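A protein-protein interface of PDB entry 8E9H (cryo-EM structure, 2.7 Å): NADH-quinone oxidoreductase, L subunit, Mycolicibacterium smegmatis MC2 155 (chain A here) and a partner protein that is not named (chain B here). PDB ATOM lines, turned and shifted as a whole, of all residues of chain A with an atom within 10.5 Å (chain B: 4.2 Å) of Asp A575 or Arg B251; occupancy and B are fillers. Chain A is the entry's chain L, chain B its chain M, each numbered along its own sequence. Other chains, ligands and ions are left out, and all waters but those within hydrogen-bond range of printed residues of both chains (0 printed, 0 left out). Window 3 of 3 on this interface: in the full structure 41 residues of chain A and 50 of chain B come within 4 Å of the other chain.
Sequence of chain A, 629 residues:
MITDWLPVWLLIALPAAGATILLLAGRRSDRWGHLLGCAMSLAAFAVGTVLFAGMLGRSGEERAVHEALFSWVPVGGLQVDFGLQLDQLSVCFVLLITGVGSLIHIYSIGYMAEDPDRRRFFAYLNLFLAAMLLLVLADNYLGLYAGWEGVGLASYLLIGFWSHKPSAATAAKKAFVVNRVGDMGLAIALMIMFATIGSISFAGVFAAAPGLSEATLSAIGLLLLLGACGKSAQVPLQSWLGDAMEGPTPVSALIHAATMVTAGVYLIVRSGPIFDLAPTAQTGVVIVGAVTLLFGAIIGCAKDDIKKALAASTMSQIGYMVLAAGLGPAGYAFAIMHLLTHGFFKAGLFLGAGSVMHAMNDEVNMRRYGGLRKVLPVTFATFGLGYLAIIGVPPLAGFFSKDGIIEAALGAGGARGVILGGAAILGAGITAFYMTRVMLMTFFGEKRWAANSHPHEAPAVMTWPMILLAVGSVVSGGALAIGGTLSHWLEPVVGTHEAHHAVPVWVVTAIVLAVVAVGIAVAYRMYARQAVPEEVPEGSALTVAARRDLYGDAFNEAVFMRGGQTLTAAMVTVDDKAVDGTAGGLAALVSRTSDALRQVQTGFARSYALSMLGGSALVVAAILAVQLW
The side-chain hydroxyl of Tyr B309 sits at hydrogen-bond distance from the side-chain carboxylate of Asp A575 (2.6 Å). OD2 of Asp A575 is in hydrogen-bond range of OH of Tyr B326, at 2.6 Å. The side-chain carboxylate of Asp A575 is in salt-bridge range of the guanidinium group of Arg B251, 3.1 Å away. The side-chain carboxylate (OD1) of Asp A575 sits at hydrogen-bond distance from a ring nitrogen (NE2) of His B250 (2.8 Å). OD1 of Asp A580 is in salt-bridge range of NZ of Lys B174 (3.8 Å).
Asp A575 touches just these residues of chain B: His B250, Arg B251, Tyr B309, Leu B313 and Tyr B326. Arg B251 touches just these residues of chain A: Asp A575 and Asp A580. Printed residues of chain B within 4 Å of Val A574: Tyr B309. Of the printed residues of chain A, Tyr B326 touches Asp A575 (2.6 Å). Of the printed residues of chain B, Val A572 touches Leu B313 (3.5 Å). Ala A578 touches none of the printed residues of chain B. Lys A577 touches none of the printed residues of chain B. The nearest printed residue of chain B that does not touch Asp A575 is Pro B254 (5.4 Å).
Hydrophobic or aromatic side chains of chain A that line the printed part of chain B: Met A571, Val A572, Val A574 and Val A579. Among the printed residues, 13 pairs touch across the chains.
Among the printed residues, merely in contact across the chains: Val A579 with Pro B248, Asp A575 with Leu B313, Met A571 with Leu B313, Asp A580 with Arg B251, Val A572 with Leu B313, Met A571 with Tyr B309, Val A579 with Tyr B309 and Val A574 with Tyr B309.
O of Val A574 lies within hydrogen-bond range of N of Val A579 (2.9 Å). N of Asp A580 is in hydrogen-bond range of O of Asp A575 (3.1 Å). The backbone carbonyl oxygen (O) of Val A579 is in hydrogen-bond range of the side-chain hydroxyl (OG1) of Thr A582, at 2.8 Å. A ring nitrogen (ND1) of His B250 is in hydrogen-bond range of the backbone carbonyl oxygen (O) of Pro B248, 3.4 Å away.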
ATOM      1  N   LEU A 567       8.077 -15.939 -37.574  1.00  0.00           N
ATOM      2  CA  LEU A 567       9.015 -15.755 -36.475  1.00  0.00           C
ATOM      3  C   LEU A 567       8.741 -16.748 -35.354  1.00  0.00           C
ATOM      4  O   LEU A 567       9.674 -17.291 -34.751  1.00  0.00           O
ATOM      5  CB  LEU A 567       8.931 -14.321 -35.953  1.00  0.00           C
ATOM      6  CG  LEU A 567       9.766 -13.997 -34.715  1.00  0.00           C
ATOM      7  CD1 LEU A 567      11.241 -14.191 -35.000  1.00  0.00           C
ATOM      8  CD2 LEU A 567       9.490 -12.579 -34.250  1.00  0.00           C
ATOM      9  N   THR A 568       7.467 -16.987 -35.051  1.00  0.00           N
ATOM     10  CA  THR A 568       7.115 -17.929 -33.996  1.00  0.00           C
ATOM     11  C   THR A 568       7.578 -19.334 -34.348  1.00  0.00           C
ATOM     12  O   THR A 568       8.117 -20.051 -33.499  1.00  0.00           O
ATOM     13  CB  THR A 568       5.607 -17.906 -33.761  1.00  0.00           C
ATOM     14  OG1 THR A 568       5.199 -16.584 -33.394  1.00  0.00           O
ATOM     15  CG2 THR A 568       5.226 -18.872 -32.657  1.00  0.00           C
ATOM     16  N   ALA A 569       7.366 -19.750 -35.595  1.00  0.00           N
ATOM     17  CA  ALA A 569       7.831 -21.067 -36.014  1.00  0.00           C
ATOM     18  C   ALA A 569       9.345 -21.157 -35.932  1.00  0.00           C
ATOM     19  O   ALA A 569       9.894 -22.174 -35.492  1.00  0.00           O
ATOM     20  CB  ALA A 569       7.350 -21.366 -37.432  1.00  0.00           C
ATOM     21  N   ALA A 570      10.042 -20.100 -36.346  1.00  0.00           N
ATOM     22  CA  ALA A 570      11.497 -20.102 -36.269  1.00  0.00           C
ATOM     23  C   ALA A 570      11.964 -20.245 -34.829  1.00  0.00           C
ATOM     24  O   ALA A 570      12.880 -21.020 -34.533  1.00  0.00           O
ATOM     25  CB  ALA A 570      12.055 -18.823 -36.891  1.00  0.00           C
ATOM     26  N   MET A 571      11.344 -19.503 -33.913  1.00  0.00           N
ATOM     27  CA  MET A 571      11.748 -19.571 -32.514  1.00  0.00           C
ATOM     28  C   MET A 571      11.426 -20.932 -31.911  1.00  0.00           C
ATOM     29  O   MET A 571      12.202 -21.458 -31.107  1.00  0.00           O
ATOM     30  CB  MET A 571      11.071 -18.457 -31.717  1.00  0.00           C
ATOM     31  CG  MET A 571      11.672 -17.066 -31.917  1.00  0.00           C
ATOM     32  SD  MET A 571      13.475 -17.016 -31.898  1.00  0.00           S
ATOM     33  CE  MET A 571      13.830 -16.744 -33.630  1.00  0.00           C
ATOM     34  N   VAL A 572      10.286 -21.517 -32.279  1.00  0.00           N
ATOM     35  CA  VAL A 572       9.959 -22.852 -31.791  1.00  0.00           C
ATOM     36  C   VAL A 572      10.987 -23.857 -32.286  1.00  0.00           C
ATOM     37  O   VAL A 572      11.424 -24.744 -31.541  1.00  0.00           O
ATOM     38  CB  VAL A 572       8.533 -23.243 -32.216  1.00  0.00           C
ATOM     39  CG1 VAL A 572       8.314 -24.733 -32.031  1.00  0.00           C
ATOM     40  CG2 VAL A 572       7.515 -22.452 -31.423  1.00  0.00           C
ATOM     41  N   THR A 573      11.384 -23.742 -33.553  1.00  0.00           N
ATOM     42  CA  THR A 573      12.416 -24.623 -34.084  1.00  0.00           C
ATOM     43  C   THR A 573      13.731 -24.429 -33.346  1.00  0.00           C
ATOM     44  O   THR A 573      14.435 -25.399 -33.057  1.00  0.00           O
ATOM     45  CB  THR A 573      12.601 -24.375 -35.578  1.00  0.00           C
ATOM     46  OG1 THR A 573      11.345 -24.523 -36.249  1.00  0.00           O
ATOM     47  CG2 THR A 573      13.604 -25.355 -36.162  1.00  0.00           C
ATOM     48  N   VAL A 574      14.085 -23.181 -33.042  1.00  0.00           N
ATOM     49  CA  VAL A 574      15.311 -22.922 -32.294  1.00  0.00           C
ATOM     50  C   VAL A 574      15.242 -23.581 -30.924  1.00  0.00           C
ATOM     51  O   VAL A 574      16.204 -24.211 -30.471  1.00  0.00           O
ATOM     52  CB  VAL A 574      15.559 -21.407 -32.185  1.00  0.00           C
ATOM     53  CG1 VAL A 574      16.640 -21.113 -31.164  1.00  0.00           C
ATOM     54  CG2 VAL A 574      15.946 -20.844 -33.536  1.00  0.00           C
ATOM     55  N   ASP A 575      14.105 -23.447 -30.243  1.00  0.00           N
ATOM     56  CA  ASP A 575      13.963 -24.045 -28.920  1.00  0.00           C
ATOM     57  C   ASP A 575      14.084 -25.561 -28.988  1.00  0.00           C
ATOM     58  O   ASP A 575      14.798 -26.174 -28.187  1.00  0.00           O
ATOM     59  CB  ASP A 575      12.621 -23.655 -28.308  1.00  0.00           C
ATOM     60  CG  ASP A 575      12.648 -23.676 -26.794  1.00  0.00           C
ATOM     61  OD1 ASP A 575      13.452 -22.922 -26.206  1.00  0.00           O
ATOM     62  OD2 ASP A 575      11.872 -24.444 -26.192  1.00  0.00           O
ATOM     63  N   ASP A 576      13.390 -26.182 -29.940  1.00  0.00           N
ATOM     64  CA  ASP A 576      13.328 -27.638 -29.976  1.00  0.00           C
ATOM     65  C   ASP A 576      14.624 -28.252 -30.491  1.00  0.00           C
ATOM     66  O   ASP A 576      15.006 -29.346 -30.062  1.00  0.00           O
ATOM     67  CB  ASP A 576      12.153 -28.088 -30.841  1.00  0.00           C
ATOM     68  N   LYS A 577      15.310 -27.569 -31.406  1.00  0.00           N
ATOM     69  CA  LYS A 577      16.462 -28.147 -32.084  1.00  0.00           C
ATOM     70  C   LYS A 577      17.782 -27.540 -31.631  1.00  0.00           C
ATOM     71  O   LYS A 577      18.793 -28.246 -31.582  1.00  0.00           O
ATOM     72  CB  LYS A 577      16.314 -27.975 -33.597  1.00  0.00           C
ATOM     73  N   ALA A 578      17.809 -26.245 -31.318  1.00  0.00           N
ATOM     74  CA  ALA A 578      19.067 -25.584 -30.979  1.00  0.00           C
ATOM     75  C   ALA A 578      19.301 -25.543 -29.472  1.00  0.00           C
ATOM     76  O   ALA A 578      20.287 -26.097 -28.976  1.00  0.00           O
ATOM     77  CB  ALA A 578      19.088 -24.168 -31.559  1.00  0.00           C
ATOM     78  N   VAL A 579      18.402 -24.896 -28.731  1.00  0.00           N
ATOM     79  CA  VAL A 579      18.591 -24.764 -27.289  1.00  0.00           C
ATOM     80  C   VAL A 579      18.550 -26.134 -26.626  1.00  0.00           C
ATOM     81  O   VAL A 579      19.523 -26.573 -26.004  1.00  0.00           O
ATOM     82  CB  VAL A 579      17.534 -23.821 -26.692  1.00  0.00           C
ATOM     83  CG1 VAL A 579      17.689 -23.742 -25.185  1.00  0.00           C
ATOM     84  CG2 VAL A 579      17.648 -22.444 -27.316  1.00  0.00           C
ATOM     85  N   ASP A 580      17.422 -26.832 -26.756  1.00  0.00           N
ATOM     86  CA  ASP A 580      17.359 -28.205 -26.276  1.00  0.00           C
ATOM     87  C   ASP A 580      18.396 -29.070 -26.972  1.00  0.00           C
ATOM     88  O   ASP A 580      18.820 -30.097 -26.429  1.00  0.00           O
ATOM     89  CB  ASP A 580      15.960 -28.772 -26.502  1.00  0.00           C
ATOM     90  CG  ASP A 580      15.754 -30.102 -25.815  1.00  0.00           C
ATOM     91  OD1 ASP A 580      15.755 -30.131 -24.568  1.00  0.00           O
ATOM     92  OD2 ASP A 580      15.591 -31.118 -26.521  1.00  0.00           O
ATOM     93  N   GLY A 581      18.813 -28.670 -28.173  1.00  0.00           N
ATOM     94  CA  GLY A 581      19.790 -29.446 -28.909  1.00  0.00           C
ATOM     95  C   GLY A 581      21.135 -29.525 -28.221  1.00  0.00           C
ATOM     96  O   GLY A 581      21.792 -30.561 -28.270  1.00  0.00           O
ATOM     97  N   THR A 582      21.575 -28.435 -27.591  1.00  0.00           N
ATOM     98  CA  THR A 582      22.861 -28.473 -26.903  1.00  0.00           C
ATOM     99  C   THR A 582      22.841 -29.473 -25.755  1.00  0.00           C
ATOM    100  O   THR A 582      23.776 -30.266 -25.597  1.00  0.00           O
ATOM    101  CB  THR A 582      23.230 -27.085 -26.387  1.00  0.00           C
ATOM    102  OG1 THR A 582      22.226 -26.629 -25.474  1.00  0.00           O
ATOM    103  CG2 THR A 582      23.351 -26.104 -27.539  1.00  0.00           C
ATOM    104  N   ALA A 583      21.784 -29.451 -24.943  1.00  0.00           N
ATOM    105  CA  ALA A 583      21.682 -30.411 -23.852  1.00  0.00           C
ATOM    106  C   ALA A 583      21.562 -31.832 -24.381  1.00  0.00           C
ATOM    107  O   ALA A 583      22.172 -32.757 -23.835  1.00  0.00           O
ATOM    108  CB  ALA A 583      20.490 -30.069 -22.964  1.00  0.00           C
ATOM    109  N   GLY A 584      20.775 -32.028 -25.438  1.00  0.00           N
ATOM    110  CA  GLY A 584      20.674 -33.353 -26.024  1.00  0.00           C
ATOM    111  C   GLY A 584      22.006 -33.853 -26.542  1.00  0.00           C
ATOM    112  O   GLY A 584      22.352 -35.021 -26.369  1.00  0.00           O
ATOM    113  N   LYS B 174      15.152 -34.154 -16.073  1.00  0.00           N
ATOM    114  CA  LYS B 174      15.682 -32.932 -16.670  1.00  0.00           C
ATOM    115  C   LYS B 174      15.707 -31.798 -15.658  1.00  0.00           C
ATOM    116  O   LYS B 174      16.712 -31.088 -15.532  1.00  0.00           O
ATOM    117  CB  LYS B 174      14.863 -32.541 -17.897  1.00  0.00           C
ATOM    118  CG  LYS B 174      15.145 -33.396 -19.118  1.00  0.00           C
ATOM    119  CD  LYS B 174      15.023 -32.594 -20.396  1.00  0.00           C
ATOM    120  CE  LYS B 174      13.647 -31.975 -20.532  1.00  0.00           C
ATOM    121  NZ  LYS B 174      13.445 -31.397 -21.884  1.00  0.00           N
ATOM    122  N   PRO B 248      19.341 -18.848 -22.228  1.00  0.00           N
ATOM    123  CA  PRO B 248      18.703 -20.027 -22.815  1.00  0.00           C
ATOM    124  C   PRO B 248      18.668 -21.244 -21.896  1.00  0.00           C
ATOM    125  O   PRO B 248      18.360 -22.341 -22.354  1.00  0.00           O
ATOM    126  CB  PRO B 248      19.580 -20.304 -24.029  1.00  0.00           C
ATOM    127  CG  PRO B 248      20.934 -19.931 -23.566  1.00  0.00           C
ATOM    128  CD  PRO B 248      20.761 -18.773 -22.613  1.00  0.00           C
ATOM    129  N   PHE B 249      18.979 -21.055 -20.616  1.00  0.00           N
ATOM    130  CA  PHE B 249      18.977 -22.154 -19.660  1.00  0.00           C
ATOM    131  C   PHE B 249      17.578 -22.542 -19.203  1.00  0.00           C
ATOM    132  O   PHE B 249      17.445 -23.272 -18.217  1.00  0.00           O
ATOM    133  CB  PHE B 249      19.832 -21.786 -18.446  1.00  0.00           C
ATOM    134  CG  PHE B 249      21.164 -21.197 -18.804  1.00  0.00           C
ATOM    135  CD1 PHE B 249      22.127 -21.966 -19.432  1.00  0.00           C
ATOM    136  CD2 PHE B 249      21.456 -19.878 -18.516  1.00  0.00           C
ATOM    137  CE1 PHE B 249      23.352 -21.432 -19.763  1.00  0.00           C
ATOM    138  CE2 PHE B 249      22.682 -19.339 -18.844  1.00  0.00           C
ATOM    139  CZ  PHE B 249      23.630 -20.116 -19.469  1.00  0.00           C
ATOM    140  N   HIS B 250      16.542 -22.078 -19.896  1.00  0.00           N
ATOM    141  CA  HIS B 250      15.161 -22.287 -19.490  1.00  0.00           C
ATOM    142  C   HIS B 250      14.612 -23.651 -19.873  1.00  0.00           C
ATOM    143  O   HIS B 250      13.554 -24.033 -19.367  1.00  0.00           O
ATOM    144  CB  HIS B 250      14.289 -21.221 -20.136  1.00  0.00           C
ATOM    145  CG  HIS B 250      14.192 -21.364 -21.621  1.00  0.00           C
ATOM    146  ND1 HIS B 250      15.201 -20.967 -22.469  1.00  0.00           N
ATOM    147  CD2 HIS B 250      13.218 -21.875 -22.409  1.00  0.00           C
ATOM    148  CE1 HIS B 250      14.849 -21.218 -23.716  1.00  0.00           C
ATOM    149  NE2 HIS B 250      13.651 -21.770 -23.707  1.00  0.00           N
ATOM    150  N   ARG B 251      15.291 -24.388 -20.746  1.00  0.00           N
ATOM    151  CA  ARG B 251      14.632 -25.474 -21.457  1.00  0.00           C
ATOM    152  C   ARG B 251      14.116 -26.569 -20.534  1.00  0.00           C
ATOM    153  O   ARG B 251      13.280 -27.369 -20.962  1.00  0.00           O
ATOM    154  CB  ARG B 251      15.592 -26.070 -22.483  1.00  0.00           C
ATOM    155  CG  ARG B 251      14.932 -26.951 -23.525  1.00  0.00           C
ATOM    156  CD  ARG B 251      13.859 -26.200 -24.304  1.00  0.00           C
ATOM    157  NE  ARG B 251      13.191 -27.061 -25.268  1.00  0.00           N
ATOM    158  CZ  ARG B 251      12.323 -28.010 -24.947  1.00  0.00           C
ATOM    159  NH1 ARG B 251      12.009 -28.262 -23.686  1.00  0.00           N
ATOM    160  NH2 ARG B 251      11.765 -28.732 -25.913  1.00  0.00           N
ATOM    161  N   TRP B 252      14.596 -26.632 -19.293  1.00  0.00           N
ATOM    162  CA  TRP B 252      14.103 -27.634 -18.357  1.00  0.00           C
ATOM    163  C   TRP B 252      12.710 -27.298 -17.846  1.00  0.00           C
ATOM    164  O   TRP B 252      11.921 -28.203 -17.562  1.00  0.00           O
ATOM    165  CB  TRP B 252      15.083 -27.761 -17.196  1.00  0.00           C
ATOM    166  CG  TRP B 252      15.271 -26.483 -16.449  1.00  0.00           C
ATOM    167  CD1 TRP B 252      16.242 -25.561 -16.671  1.00  0.00           C
ATOM    168  CD2 TRP B 252      14.498 -25.995 -15.345  1.00  0.00           C
ATOM    169  NE1 TRP B 252      16.111 -24.514 -15.795  1.00  0.00           N
ATOM    170  CE2 TRP B 252      15.052 -24.762 -14.964  1.00  0.00           C
ATOM    171  CE3 TRP B 252      13.393 -26.481 -14.639  1.00  0.00           C
ATOM    172  CZ2 TRP B 252      14.537 -24.004 -13.919  1.00  0.00           C
ATOM    173  CZ3 TRP B 252      12.881 -25.722 -13.601  1.00  0.00           C
ATOM    174  CH2 TRP B 252      13.455 -24.502 -13.249  1.00  0.00           C
ATOM    175  N   LEU B 253      12.390 -26.019 -17.726  1.00  0.00           N
ATOM    176  CA  LEU B 253      11.176 -25.617 -17.033  1.00  0.00           C
ATOM    177  C   LEU B 253       9.904 -26.067 -17.743  1.00  0.00           C
ATOM    178  O   LEU B 253       8.983 -26.548 -17.078  1.00  0.00           O
ATOM    179  CB  LEU B 253      11.139 -24.102 -16.841  1.00  0.00           C
ATOM    180  CG  LEU B 253       9.822 -23.595 -16.257  1.00  0.00           C
ATOM    181  CD1 LEU B 253       9.449 -24.353 -14.988  1.00  0.00           C
ATOM    182  CD2 LEU B 253       9.933 -22.123 -15.960  1.00  0.00           C
ATOM    183  N   PRO B 254       9.777 -25.899 -19.061  1.00  0.00           N
ATOM    184  CA  PRO B 254       8.503 -26.273 -19.697  1.00  0.00           C
ATOM    185  C   PRO B 254       8.097 -27.710 -19.428  1.00  0.00           C
ATOM    186  O   PRO B 254       6.940 -27.970 -19.069  1.00  0.00           O
ATOM    187  CB  PRO B 254       8.775 -26.026 -21.184  1.00  0.00           C
ATOM    188  CG  PRO B 254       9.838 -25.006 -21.207  1.00  0.00           C
ATOM    189  CD  PRO B 254      10.713 -25.307 -20.031  1.00  0.00           C
ATOM    190  N   TYR B 309      11.790 -13.984 -26.283  1.00  0.00           N
ATOM    191  CA  TYR B 309      11.802 -15.355 -26.773  1.00  0.00           C
ATOM    192  C   TYR B 309      10.749 -16.202 -26.075  1.00  0.00           C
ATOM    193  O   TYR B 309      10.042 -16.987 -26.715  1.00  0.00           O
ATOM    194  CB  TYR B 309      13.205 -15.919 -26.558  1.00  0.00           C
ATOM    195  CG  TYR B 309      13.431 -17.344 -26.977  1.00  0.00           C
ATOM    196  CD1 TYR B 309      13.271 -18.382 -26.076  1.00  0.00           C
ATOM    197  CD2 TYR B 309      13.844 -17.649 -28.263  1.00  0.00           C
ATOM    198  CE1 TYR B 309      13.501 -19.683 -26.446  1.00  0.00           C
ATOM    199  CE2 TYR B 309      14.070 -18.947 -28.645  1.00  0.00           C
ATOM    200  CZ  TYR B 309      13.897 -19.961 -27.733  1.00  0.00           C
ATOM    201  OH  TYR B 309      14.126 -21.261 -28.108  1.00  0.00           O
ATOM    202  N   LEU B 313       7.578 -17.985 -27.860  1.00  0.00           N
ATOM    203  CA  LEU B 313       7.300 -19.410 -27.732  1.00  0.00           C
ATOM    204  C   LEU B 313       5.917 -19.641 -27.144  1.00  0.00           C
ATOM    205  O   LEU B 313       5.165 -20.493 -27.631  1.00  0.00           O
ATOM    206  CB  LEU B 313       8.366 -20.082 -26.872  1.00  0.00           C
ATOM    207  CG  LEU B 313       9.754 -20.225 -27.498  1.00  0.00           C
ATOM    208  CD1 LEU B 313      10.599 -21.152 -26.659  1.00  0.00           C
ATOM    209  CD2 LEU B 313       9.686 -20.726 -28.928  1.00  0.00           C
ATOM    210  N   TYR B 326       6.153 -20.922 -20.522  1.00  0.00           N
ATOM    211  CA  TYR B 326       6.955 -19.960 -21.268  1.00  0.00           C
ATOM    212  C   TYR B 326       6.625 -18.529 -20.868  1.00  0.00           C
ATOM    213  O   TYR B 326       7.513 -17.666 -20.854  1.00  0.00           O
ATOM    214  CB  TYR B 326       6.765 -20.174 -22.764  1.00  0.00           C
ATOM    215  CG  TYR B 326       7.568 -21.339 -23.279  1.00  0.00           C
ATOM    216  CD1 TYR B 326       8.951 -21.284 -23.316  1.00  0.00           C
ATOM    217  CD2 TYR B 326       6.949 -22.498 -23.711  1.00  0.00           C
ATOM    218  CE1 TYR B 326       9.693 -22.344 -23.776  1.00  0.00           C
ATOM    219  CE2 TYR B 326       7.684 -23.564 -24.176  1.00  0.00           C
ATOM    220  CZ  TYR B 326       9.057 -23.481 -24.205  1.00  0.00           C
ATOM    221  OH  TYR B 326       9.799 -24.542 -24.667  1.00  0.00           O
